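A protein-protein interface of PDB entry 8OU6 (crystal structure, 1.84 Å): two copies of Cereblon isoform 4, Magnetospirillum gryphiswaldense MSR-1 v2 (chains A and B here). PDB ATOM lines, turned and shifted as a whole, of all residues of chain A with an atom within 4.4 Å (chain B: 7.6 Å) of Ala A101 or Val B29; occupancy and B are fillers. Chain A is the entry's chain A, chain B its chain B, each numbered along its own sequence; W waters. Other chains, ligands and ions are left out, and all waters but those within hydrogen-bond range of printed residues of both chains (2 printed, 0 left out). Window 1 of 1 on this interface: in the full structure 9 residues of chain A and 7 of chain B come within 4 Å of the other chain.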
ATOM      1  N   ILE A   3      20.683 -28.042  17.540  1.00  0.00           N
ATOM      2  CA  ILE A   3      20.901 -29.440  17.880  1.00  0.00           C
ATOM      3  C   ILE A   3      20.395 -29.597  19.307  1.00  0.00           C
ATOM      4  O   ILE A   3      20.523 -28.666  20.102  1.00  0.00           O
ATOM      5  CB  ILE A   3      22.408 -29.801  17.848  1.00  0.00           C
ATOM      6  CG1 ILE A   3      23.063 -29.550  16.489  1.00  0.00           C
ATOM      7  CG2 ILE A   3      22.671 -31.222  18.302  1.00  0.00           C
ATOM      8  CD1 ILE A   3      22.351 -30.161  15.332  1.00  0.00           C
ATOM      9  N   PHE A   4      19.813 -30.754  19.591  1.00  0.00           N
ATOM     10  CA  PHE A   4      19.500 -31.198  20.933  1.00  0.00           C
ATOM     11  C   PHE A   4      20.508 -32.260  21.358  1.00  0.00           C
ATOM     12  O   PHE A   4      20.714 -33.247  20.663  1.00  0.00           O
ATOM     13  CB  PHE A   4      18.076 -31.739  20.972  1.00  0.00           C
ATOM     14  CG  PHE A   4      17.018 -30.698  20.745  1.00  0.00           C
ATOM     15  CD1 PHE A   4      16.661 -29.814  21.752  1.00  0.00           C
ATOM     16  CD2 PHE A   4      16.436 -30.528  19.494  1.00  0.00           C
ATOM     17  CE1 PHE A   4      15.711 -28.828  21.526  1.00  0.00           C
ATOM     18  CE2 PHE A   4      15.446 -29.574  19.293  1.00  0.00           C
ATOM     19  CZ  PHE A   4      15.123 -28.699  20.295  1.00  0.00           C
ATOM     20  N   ARG A   5      21.097 -32.041  22.546  1.00  0.00           N
ATOM     21  CA  ARG A   5      22.022 -32.953  23.185  1.00  0.00           C
ATOM     22  C   ARG A   5      21.430 -33.426  24.501  1.00  0.00           C
ATOM     23  O   ARG A   5      20.547 -32.791  25.002  1.00  0.00           O
ATOM     24  CB  ARG A   5      23.354 -32.245  23.419  1.00  0.00           C
ATOM     25  CG  ARG A   5      24.121 -32.010  22.123  1.00  0.00           C
ATOM     26  CD  ARG A   5      25.490 -31.401  22.360  1.00  0.00           C
ATOM     27  NE  ARG A   5      26.138 -31.194  21.075  1.00  0.00           N
ATOM     28  CZ  ARG A   5      26.595 -32.170  20.299  1.00  0.00           C
ATOM     29  NH1 ARG A   5      26.662 -33.403  20.770  1.00  0.00           N
ATOM     30  NH2 ARG A   5      26.967 -31.906  19.065  1.00  0.00           N
ATOM     31  N   ARG A   7      21.191 -33.505  28.236  1.00  0.00           N
ATOM     32  CA  ARG A   7      21.594 -32.530  29.234  1.00  0.00           C
ATOM     33  C   ARG A   7      22.640 -33.077  30.221  1.00  0.00           C
ATOM     34  O   ARG A   7      23.390 -32.280  30.799  1.00  0.00           O
ATOM     35  CB  ARG A   7      20.321 -32.008  29.915  1.00  0.00           C
ATOM     36  CG  ARG A   7      20.545 -31.210  31.183  1.00  0.00           C
ATOM     37  CD  ARG A   7      19.195 -30.925  31.803  1.00  0.00           C
ATOM     38  NE  ARG A   7      19.394 -30.008  32.890  1.00  0.00           N
ATOM     39  CZ  ARG A   7      18.445 -29.535  33.663  1.00  0.00           C
ATOM     40  NH1 ARG A   7      17.168 -29.759  33.383  1.00  0.00           N
ATOM     41  NH2 ARG A   7      18.800 -28.823  34.716  1.00  0.00           N
ATOM     42  N   ASP A  98      13.027 -31.129  29.150  1.00  0.00           N
ATOM     43  CA  ASP A  98      14.017 -30.573  30.088  1.00  0.00           C
ATOM     44  C   ASP A  98      15.153 -31.554  30.380  1.00  0.00           C
ATOM     45  O   ASP A  98      16.030 -31.252  31.191  1.00  0.00           O
ATOM     46  CB  ASP A  98      13.377 -30.054  31.377  1.00  0.00           C
ATOM     47  CG  ASP A  98      12.800 -31.159  32.233  1.00  0.00           C
ATOM     48  OD1 ASP A  98      12.112 -31.982  31.670  1.00  0.00           O
ATOM     49  OD2 ASP A  98      13.025 -31.154  33.455  1.00  0.00           O
ATOM     50  N   LEU A 100      16.907 -32.463  27.721  1.00  0.00           N
ATOM     51  CA  LEU A 100      17.739 -32.120  26.580  1.00  0.00           C
ATOM     52  C   LEU A 100      18.298 -30.709  26.786  1.00  0.00           C
ATOM     53  O   LEU A 100      17.759 -29.956  27.582  1.00  0.00           O
ATOM     54  CB  LEU A 100      16.894 -32.123  25.313  1.00  0.00           C
ATOM     55  CG  LEU A 100      16.201 -33.448  24.983  1.00  0.00           C
ATOM     56  CD1 LEU A 100      15.299 -33.260  23.776  1.00  0.00           C
ATOM     57  CD2 LEU A 100      17.232 -34.542  24.740  1.00  0.00           C
ATOM     58  N   ALA A 101      19.383 -30.390  26.073  1.00  0.00           N
ATOM     59  CA  ALA A 101      19.950 -29.049  25.970  1.00  0.00           C
ATOM     60  C   ALA A 101      20.034 -28.686  24.485  1.00  0.00           C
ATOM     61  O   ALA A 101      20.520 -29.479  23.671  1.00  0.00           O
ATOM     62  CB  ALA A 101      21.320 -28.973  26.598  1.00  0.00           C
ATOM     63  N   GLU A 102      19.616 -27.452  24.154  1.00  0.00           N
ATOM     64  CA  GLU A 102      19.556 -26.998  22.783  1.00  0.00           C
ATOM     65  C   GLU A 102      20.739 -26.087  22.500  1.00  0.00           C
ATOM     66  O   GLU A 102      21.025 -25.224  23.313  1.00  0.00           O
ATOM     67  CB  GLU A 102      18.266 -26.210  22.570  1.00  0.00           C
ATOM     68  CG  GLU A 102      17.993 -25.906  21.109  1.00  0.00           C
ATOM     69  CD  GLU A 102      16.605 -25.328  20.818  1.00  0.00           C
ATOM     70  OE1 GLU A 102      15.793 -25.166  21.778  1.00  0.00           O
ATOM     71  OE2 GLU A 102      16.321 -25.054  19.635  1.00  0.00           O
ATOM     72  N   GLY A 103      21.357 -26.229  21.327  1.00  0.00           N
ATOM     73  CA  GLY A 103      22.469 -25.354  21.001  1.00  0.00           C
ATOM     74  C   GLY A 103      22.994 -25.470  19.574  1.00  0.00           C
ATOM     75  O   GLY A 103      22.395 -26.109  18.701  1.00  0.00           O
ATOM     76  N   ASP B  25       8.010 -21.467  26.777  1.00  0.00           N
ATOM     77  CA  ASP B  25       8.452 -21.812  28.130  1.00  0.00           C
ATOM     78  C   ASP B  25       9.393 -20.735  28.641  1.00  0.00           C
ATOM     79  O   ASP B  25      10.152 -20.186  27.851  1.00  0.00           O
ATOM     80  CB  ASP B  25       9.107 -23.198  28.114  1.00  0.00           C
ATOM     81  CG  ASP B  25       9.290 -23.884  29.464  1.00  0.00           C
ATOM     82  OD1 ASP B  25       9.204 -23.224  30.516  1.00  0.00           O
ATOM     83  OD2 ASP B  25       9.522 -25.092  29.444  1.00  0.00           O
ATOM     84  N   HIS B  26       9.355 -20.436  29.950  1.00  0.00           N
ATOM     85  CA  HIS B  26      10.317 -19.494  30.503  1.00  0.00           C
ATOM     86  C   HIS B  26      11.657 -20.186  30.754  1.00  0.00           C
ATOM     87  O   HIS B  26      12.665 -19.508  30.812  1.00  0.00           O
ATOM     88  CB  HIS B  26       9.786 -18.780  31.743  1.00  0.00           C
ATOM     89  CG  HIS B  26       9.624 -19.655  32.927  1.00  0.00           C
ATOM     90  ND1 HIS B  26       8.408 -20.150  33.328  1.00  0.00           N
ATOM     91  CD2 HIS B  26      10.541 -20.184  33.777  1.00  0.00           C
ATOM     92  CE1 HIS B  26       8.591 -20.952  34.374  1.00  0.00           C
ATOM     93  NE2 HIS B  26       9.875 -20.969  34.674  1.00  0.00           N
ATOM     94  N   GLU B  27      11.674 -21.522  30.877  1.00  0.00           N
ATOM     95  CA  GLU B  27      12.903 -22.282  31.076  1.00  0.00           C
ATOM     96  C   GLU B  27      13.460 -22.846  29.764  1.00  0.00           C
ATOM     97  O   GLU B  27      12.750 -23.521  28.988  1.00  0.00           O
ATOM     98  CB  GLU B  27      12.688 -23.425  32.052  1.00  0.00           C
ATOM     99  CG  GLU B  27      13.978 -24.173  32.346  1.00  0.00           C
ATOM    100  CD  GLU B  27      13.905 -25.222  33.435  1.00  0.00           C
ATOM    101  OE1 GLU B  27      13.874 -24.847  34.644  1.00  0.00           O
ATOM    102  OE2 GLU B  27      13.920 -26.417  33.074  1.00  0.00           O
ATOM    103  N   HIS B  28      14.726 -22.537  29.497  1.00  0.00           N
ATOM    104  CA  HIS B  28      15.451 -23.074  28.351  1.00  0.00           C
ATOM    105  C   HIS B  28      16.757 -23.714  28.824  1.00  0.00           C
ATOM    106  O   HIS B  28      17.592 -23.063  29.451  1.00  0.00           O
ATOM    107  CB  HIS B  28      15.716 -21.978  27.322  1.00  0.00           C
ATOM    108  CG  HIS B  28      14.449 -21.468  26.734  1.00  0.00           C
ATOM    109  ND1 HIS B  28      14.091 -21.703  25.428  1.00  0.00           N
ATOM    110  CD2 HIS B  28      13.458 -20.725  27.267  1.00  0.00           C
ATOM    111  CE1 HIS B  28      12.906 -21.165  25.195  1.00  0.00           C
ATOM    112  NE2 HIS B  28      12.497 -20.579  26.289  1.00  0.00           N
ATOM    113  N   VAL B  29      16.945 -25.013  28.585  1.00  0.00           N
ATOM    114  CA  VAL B  29      18.260 -25.613  28.813  1.00  0.00           C
ATOM    115  C   VAL B  29      19.045 -25.547  27.505  1.00  0.00           C
ATOM    116  O   VAL B  29      18.600 -26.053  26.482  1.00  0.00           O
ATOM    117  CB  VAL B  29      18.144 -27.049  29.352  1.00  0.00           C
ATOM    118  CG1 VAL B  29      19.515 -27.665  29.635  1.00  0.00           C
ATOM    119  CG2 VAL B  29      17.254 -27.106  30.586  1.00  0.00           C
ATOM    120  N   VAL B  30      20.227 -24.925  27.551  1.00  0.00           N
ATOM    121  CA  VAL B  30      20.969 -24.570  26.357  1.00  0.00           C
ATOM    122  C   VAL B  30      22.437 -24.966  26.546  1.00  0.00           C
ATOM    123  O   VAL B  30      22.914 -25.116  27.671  1.00  0.00           O
ATOM    124  CB  VAL B  30      20.832 -23.071  26.049  1.00  0.00           C
ATOM    125  CG1 VAL B  30      19.423 -22.692  25.593  1.00  0.00           C
ATOM    126  CG2 VAL B  30      21.254 -22.225  27.241  1.00  0.00           C
ATOM    127  N   PHE B  31      23.175 -25.090  25.435  1.00  0.00           N
ATOM    128  CA  PHE B  31      24.625 -25.259  25.518  1.00  0.00           C
ATOM    129  C   PHE B  31      25.299 -24.302  24.530  1.00  0.00           C
ATOM    130  O   PHE B  31      24.742 -23.950  23.515  1.00  0.00           O
ATOM    131  CB  PHE B  31      25.077 -26.711  25.268  1.00  0.00           C
ATOM    132  CG  PHE B  31      24.811 -27.254  23.884  1.00  0.00           C
ATOM    133  CD1 PHE B  31      25.719 -27.076  22.826  1.00  0.00           C
ATOM    134  CD2 PHE B  31      23.645 -27.964  23.627  1.00  0.00           C
ATOM    135  CE1 PHE B  31      25.445 -27.546  21.556  1.00  0.00           C
ATOM    136  CE2 PHE B  31      23.381 -28.422  22.346  1.00  0.00           C
ATOM    137  CZ  PHE B  31      24.275 -28.227  21.324  1.00  0.00           C
ATOM    138  N   ASN B  32      26.458 -23.779  24.929  1.00  0.00           N
ATOM    139  CA  ASN B  32      27.202 -22.836  24.108  1.00  0.00           C
ATOM    140  C   ASN B  32      28.212 -23.614  23.247  1.00  0.00           C
ATOM    141  O   ASN B  32      28.337 -24.828  23.335  1.00  0.00           O
ATOM    142  CB  ASN B  32      27.819 -21.762  25.014  1.00  0.00           C
ATOM    143  CG  ASN B  32      28.994 -22.202  25.863  1.00  0.00           C
ATOM    144  OD1 ASN B  32      29.523 -23.301  25.730  1.00  0.00           O
ATOM    145  ND2 ASN B  32      29.405 -21.324  26.772  1.00  0.00           N
ATOM    146  N   MET B  36      29.372 -25.783  27.304  1.00  0.00           N
ATOM    147  CA  MET B  36      28.886 -25.544  28.646  1.00  0.00           C
ATOM    148  C   MET B  36      27.358 -25.465  28.605  1.00  0.00           C
ATOM    149  O   MET B  36      26.792 -24.832  27.715  1.00  0.00           O
ATOM    150  CB  MET B  36      29.459 -24.245  29.212  1.00  0.00           C
ATOM    151  CG  MET B  36      30.971 -24.163  29.110  1.00  0.00           C
ATOM    152  SD  MET B  36      31.520 -22.477  29.581  1.00  0.00           S
ATOM    153  CE  MET B  36      32.765 -22.079  28.354  1.00  0.00           C
ATOM    154  N   ILE B  37      26.712 -26.165  29.546  1.00  0.00           N
ATOM    155  CA  ILE B  37      25.261 -26.245  29.597  1.00  0.00           C
ATOM    156  C   ILE B  37      24.725 -25.312  30.682  1.00  0.00           C
ATOM    157  O   ILE B  37      25.245 -25.260  31.778  1.00  0.00           O
ATOM    158  CB  ILE B  37      24.804 -27.700  29.828  1.00  0.00           C
ATOM    159  CG1 ILE B  37      25.252 -28.598  28.672  1.00  0.00           C
ATOM    160  CG2 ILE B  37      23.286 -27.733  30.030  1.00  0.00           C
ATOM    161  CD1 ILE B  37      24.914 -30.092  28.798  1.00  0.00           C
ATOM    162  N   PHE B  38      23.691 -24.532  30.347  1.00  0.00           N
ATOM    163  CA  PHE B  38      23.079 -23.594  31.281  1.00  0.00           C
ATOM    164  C   PHE B  38      21.583 -23.849  31.293  1.00  0.00           C
ATOM    165  O   PHE B  38      21.003 -24.108  30.226  1.00  0.00           O
ATOM    166  CB  PHE B  38      23.319 -22.146  30.847  1.00  0.00           C
ATOM    167  CG  PHE B  38      24.776 -21.742  30.716  1.00  0.00           C
ATOM    168  CD1 PHE B  38      25.475 -21.267  31.809  1.00  0.00           C
ATOM    169  CD2 PHE B  38      25.441 -21.844  29.505  1.00  0.00           C
ATOM    170  CE1 PHE B  38      26.799 -20.872  31.699  1.00  0.00           C
ATOM    171  CE2 PHE B  38      26.771 -21.455  29.401  1.00  0.00           C
ATOM    172  CZ  PHE B  38      27.441 -20.972  30.490  1.00  0.00           C
ATOM    173  N   ARG B  39      20.977 -23.787  32.484  1.00  0.00           N
ATOM    174  CA  ARG B  39      19.528 -23.702  32.590  1.00  0.00           C
ATOM    175  C   ARG B  39      19.140 -22.225  32.731  1.00  0.00           C
ATOM    176  O   ARG B  39      19.413 -21.598  33.747  1.00  0.00           O
ATOM    177  CB  ARG B  39      19.041 -24.574  33.758  1.00  0.00           C
ATOM    178  CG  ARG B  39      17.537 -24.693  33.836  1.00  0.00           C
ATOM    179  CD  ARG B  39      17.069 -25.828  34.741  1.00  0.00           C
ATOM    180  NE  ARG B  39      17.596 -25.659  36.079  1.00  0.00           N
ATOM    181  CZ  ARG B  39      16.880 -25.241  37.120  1.00  0.00           C
ATOM    182  NH1 ARG B  39      15.610 -24.896  36.978  1.00  0.00           N
ATOM    183  NH2 ARG B  39      17.469 -25.129  38.289  1.00  0.00           N
ATOM    184  N   VAL B  40      18.503 -21.684  31.687  1.00  0.00           N
ATOM    185  CA  VAL B  40      18.218 -20.262  31.551  1.00  0.00           C
ATOM    186  C   VAL B  40      16.735 -20.047  31.822  1.00  0.00           C
ATOM    187  O   VAL B  40      15.891 -20.777  31.305  1.00  0.00           O
ATOM    188  CB  VAL B  40      18.644 -19.793  30.139  1.00  0.00           C
ATOM    189  CG1 VAL B  40      18.154 -18.406  29.801  1.00  0.00           C
ATOM    190  CG2 VAL B  40      20.160 -19.861  29.995  1.00  0.00           C
ATOM    191  N   TRP B  41      16.425 -19.072  32.672  1.00  0.00           N
ATOM    192  CA  TRP B  41      15.068 -18.573  32.800  1.00  0.00           C
ATOM    193  C   TRP B  41      14.957 -17.198  32.136  1.00  0.00           C
ATOM    194  O   TRP B  41      15.780 -16.339  32.367  1.00  0.00           O
ATOM    195  CB  TRP B  41      14.631 -18.505  34.265  1.00  0.00           C
ATOM    196  CG  TRP B  41      14.238 -19.847  34.792  1.00  0.00           C
ATOM    197  CD1 TRP B  41      14.560 -21.076  34.289  1.00  0.00           C
ATOM    198  CD2 TRP B  41      13.396 -20.093  35.928  1.00  0.00           C
ATOM    199  NE1 TRP B  41      13.980 -22.076  35.043  1.00  0.00           N
ATOM    200  CE2 TRP B  41      13.259 -21.505  36.048  1.00  0.00           C
ATOM    201  CE3 TRP B  41      12.762 -19.266  36.851  1.00  0.00           C
ATOM    202  CZ2 TRP B  41      12.491 -22.085  37.061  1.00  0.00           C
ATOM    203  CZ3 TRP B  41      11.973 -19.843  37.825  1.00  0.00           C
ATOM    204  CH2 TRP B  41      11.810 -21.230  37.896  1.00  0.00           C
ATOM    205  N   TRP B  61      21.083 -18.170  21.189  1.00  0.00           N
ATOM    206  CA  TRP B  61      20.096 -19.210  21.417  1.00  0.00           C
ATOM    207  C   TRP B  61      18.711 -18.814  20.925  1.00  0.00           C
ATOM    208  O   TRP B  61      17.835 -19.659  20.777  1.00  0.00           O
ATOM    209  CB  TRP B  61      20.026 -19.594  22.893  1.00  0.00           C
ATOM    210  CG  TRP B  61      21.273 -20.284  23.353  1.00  0.00           C
ATOM    211  CD1 TRP B  61      21.894 -21.331  22.733  1.00  0.00           C
ATOM    212  CD2 TRP B  61      22.078 -19.942  24.480  1.00  0.00           C
ATOM    213  NE1 TRP B  61      22.988 -21.704  23.452  1.00  0.00           N
ATOM    214  CE2 TRP B  61      23.139 -20.872  24.518  1.00  0.00           C
ATOM    215  CE3 TRP B  61      21.960 -19.021  25.529  1.00  0.00           C
ATOM    216  CZ2 TRP B  61      24.119 -20.835  25.505  1.00  0.00           C
ATOM    217  CZ3 TRP B  61      22.943 -18.963  26.487  1.00  0.00           C
ATOM    218  CH2 TRP B  61      23.984 -19.895  26.506  1.00  0.00           C
HETATM  219  O   HOH W   1      20.265 -26.498  36.877  1.00  0.00           O
HETATM  220  O   HOH W   2      14.816 -28.388  34.583  1.00  0.00           O
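Hydrophobic or aromatic side chains of chain A that line the printed part of chain B: Ala A101. Hydrophobic or aromatic side chains of chain B within 4 Å of the printed part of chain A: Val B29, Val B30, Phe B31 and Ile B37.
The backbone carbonyl oxygen (O) of Val B29 is in hydrogen-bond range of the backbone NH (N) of Glu A102. The backbone carbonyl oxygen (O) of Glu A102 is in hydrogen-bond range of the backbone NH (N) of Phe B31 (3.0 Å).
Among the printed residues, merely in contact across the chains: Ile A3 with Phe B31 (3.6 Å), Arg A5 with Phe B31 (3.5 Å), Arg A7 with Val B29 (3.9 Å), Arg A7 with Ile B37 (3.3 Å), Arg A7 with Arg B39 (3.5 Å), Leu A100 with Val B29 (3.4 Å), Ala A101 with Val B29 (3.3 Å), Ala A101 with Phe B31 (3.3 Å), Glu A102 with Val B30 (3.1 Å) and Gly A103 with Phe B31 (3.2 Å).
Water W2 lies within hydrogen-bond range of OE2 of Glu B27 (2.6 Å), NH1 of Arg A7 (3.0 Å) and OD2 of Asp A98 (3.5 Å). Water W1 bridges the guanidinium group of Arg B39 (2.9 Å) and the guanidinium group of Arg A7 (3.5 Å).
Of chain B, only Val B29 and Phe B31 come within 4 Å of Ala A101. Printed residues of chain A within 4 Å of Arg B39: Arg A7. Printed residues of chain B within 4 Å of Ile A3: Phe B31 (3.6 Å). Of the printed residues of chain B, Leu A100 touches Val B29 (3.4 Å). Of the printed residues of chain B, Arg A5 touches Phe B31 (3.5 Å). The nearest printed residue of chain B that does not touch Ala A101 is Ile B37 (4.1 Å). The nearest printed residue of chain B that does not touch Ile A3 is Val B29 (7.2 Å).
The backbone NH (N) of Phe B38 lies within hydrogen-bond range of the backbone carbonyl oxygen (O) of Val B30 (2.8 Å). The indole nitrogen of Trp B61 lies within hydrogen-bond range of the backbone carbonyl oxygen of Phe B31 (2.9 Å). The backbone carbonyl oxygen (O) of Ala A101 sits at hydrogen-bond distance from the backbone NH (N) of Arg A5 (2.9 Å). NH1 of Arg A7 lies within hydrogen-bond range of O of Asp A98. The backbone NH (N) of Ile A3 lies within hydrogen-bond range of the backbone carbonyl oxygen (O) of Gly A103 (2.8 Å). The guanidinium group (NH1) of Arg B39 is in salt-bridge range of the side-chain carboxylate (OE1) of Glu B27, 2.9 Å away.
No position is printed for both chains. Of the 12 pairs that touch across the chains among the printed residues, none has its exchanged pair printed and touching as well.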
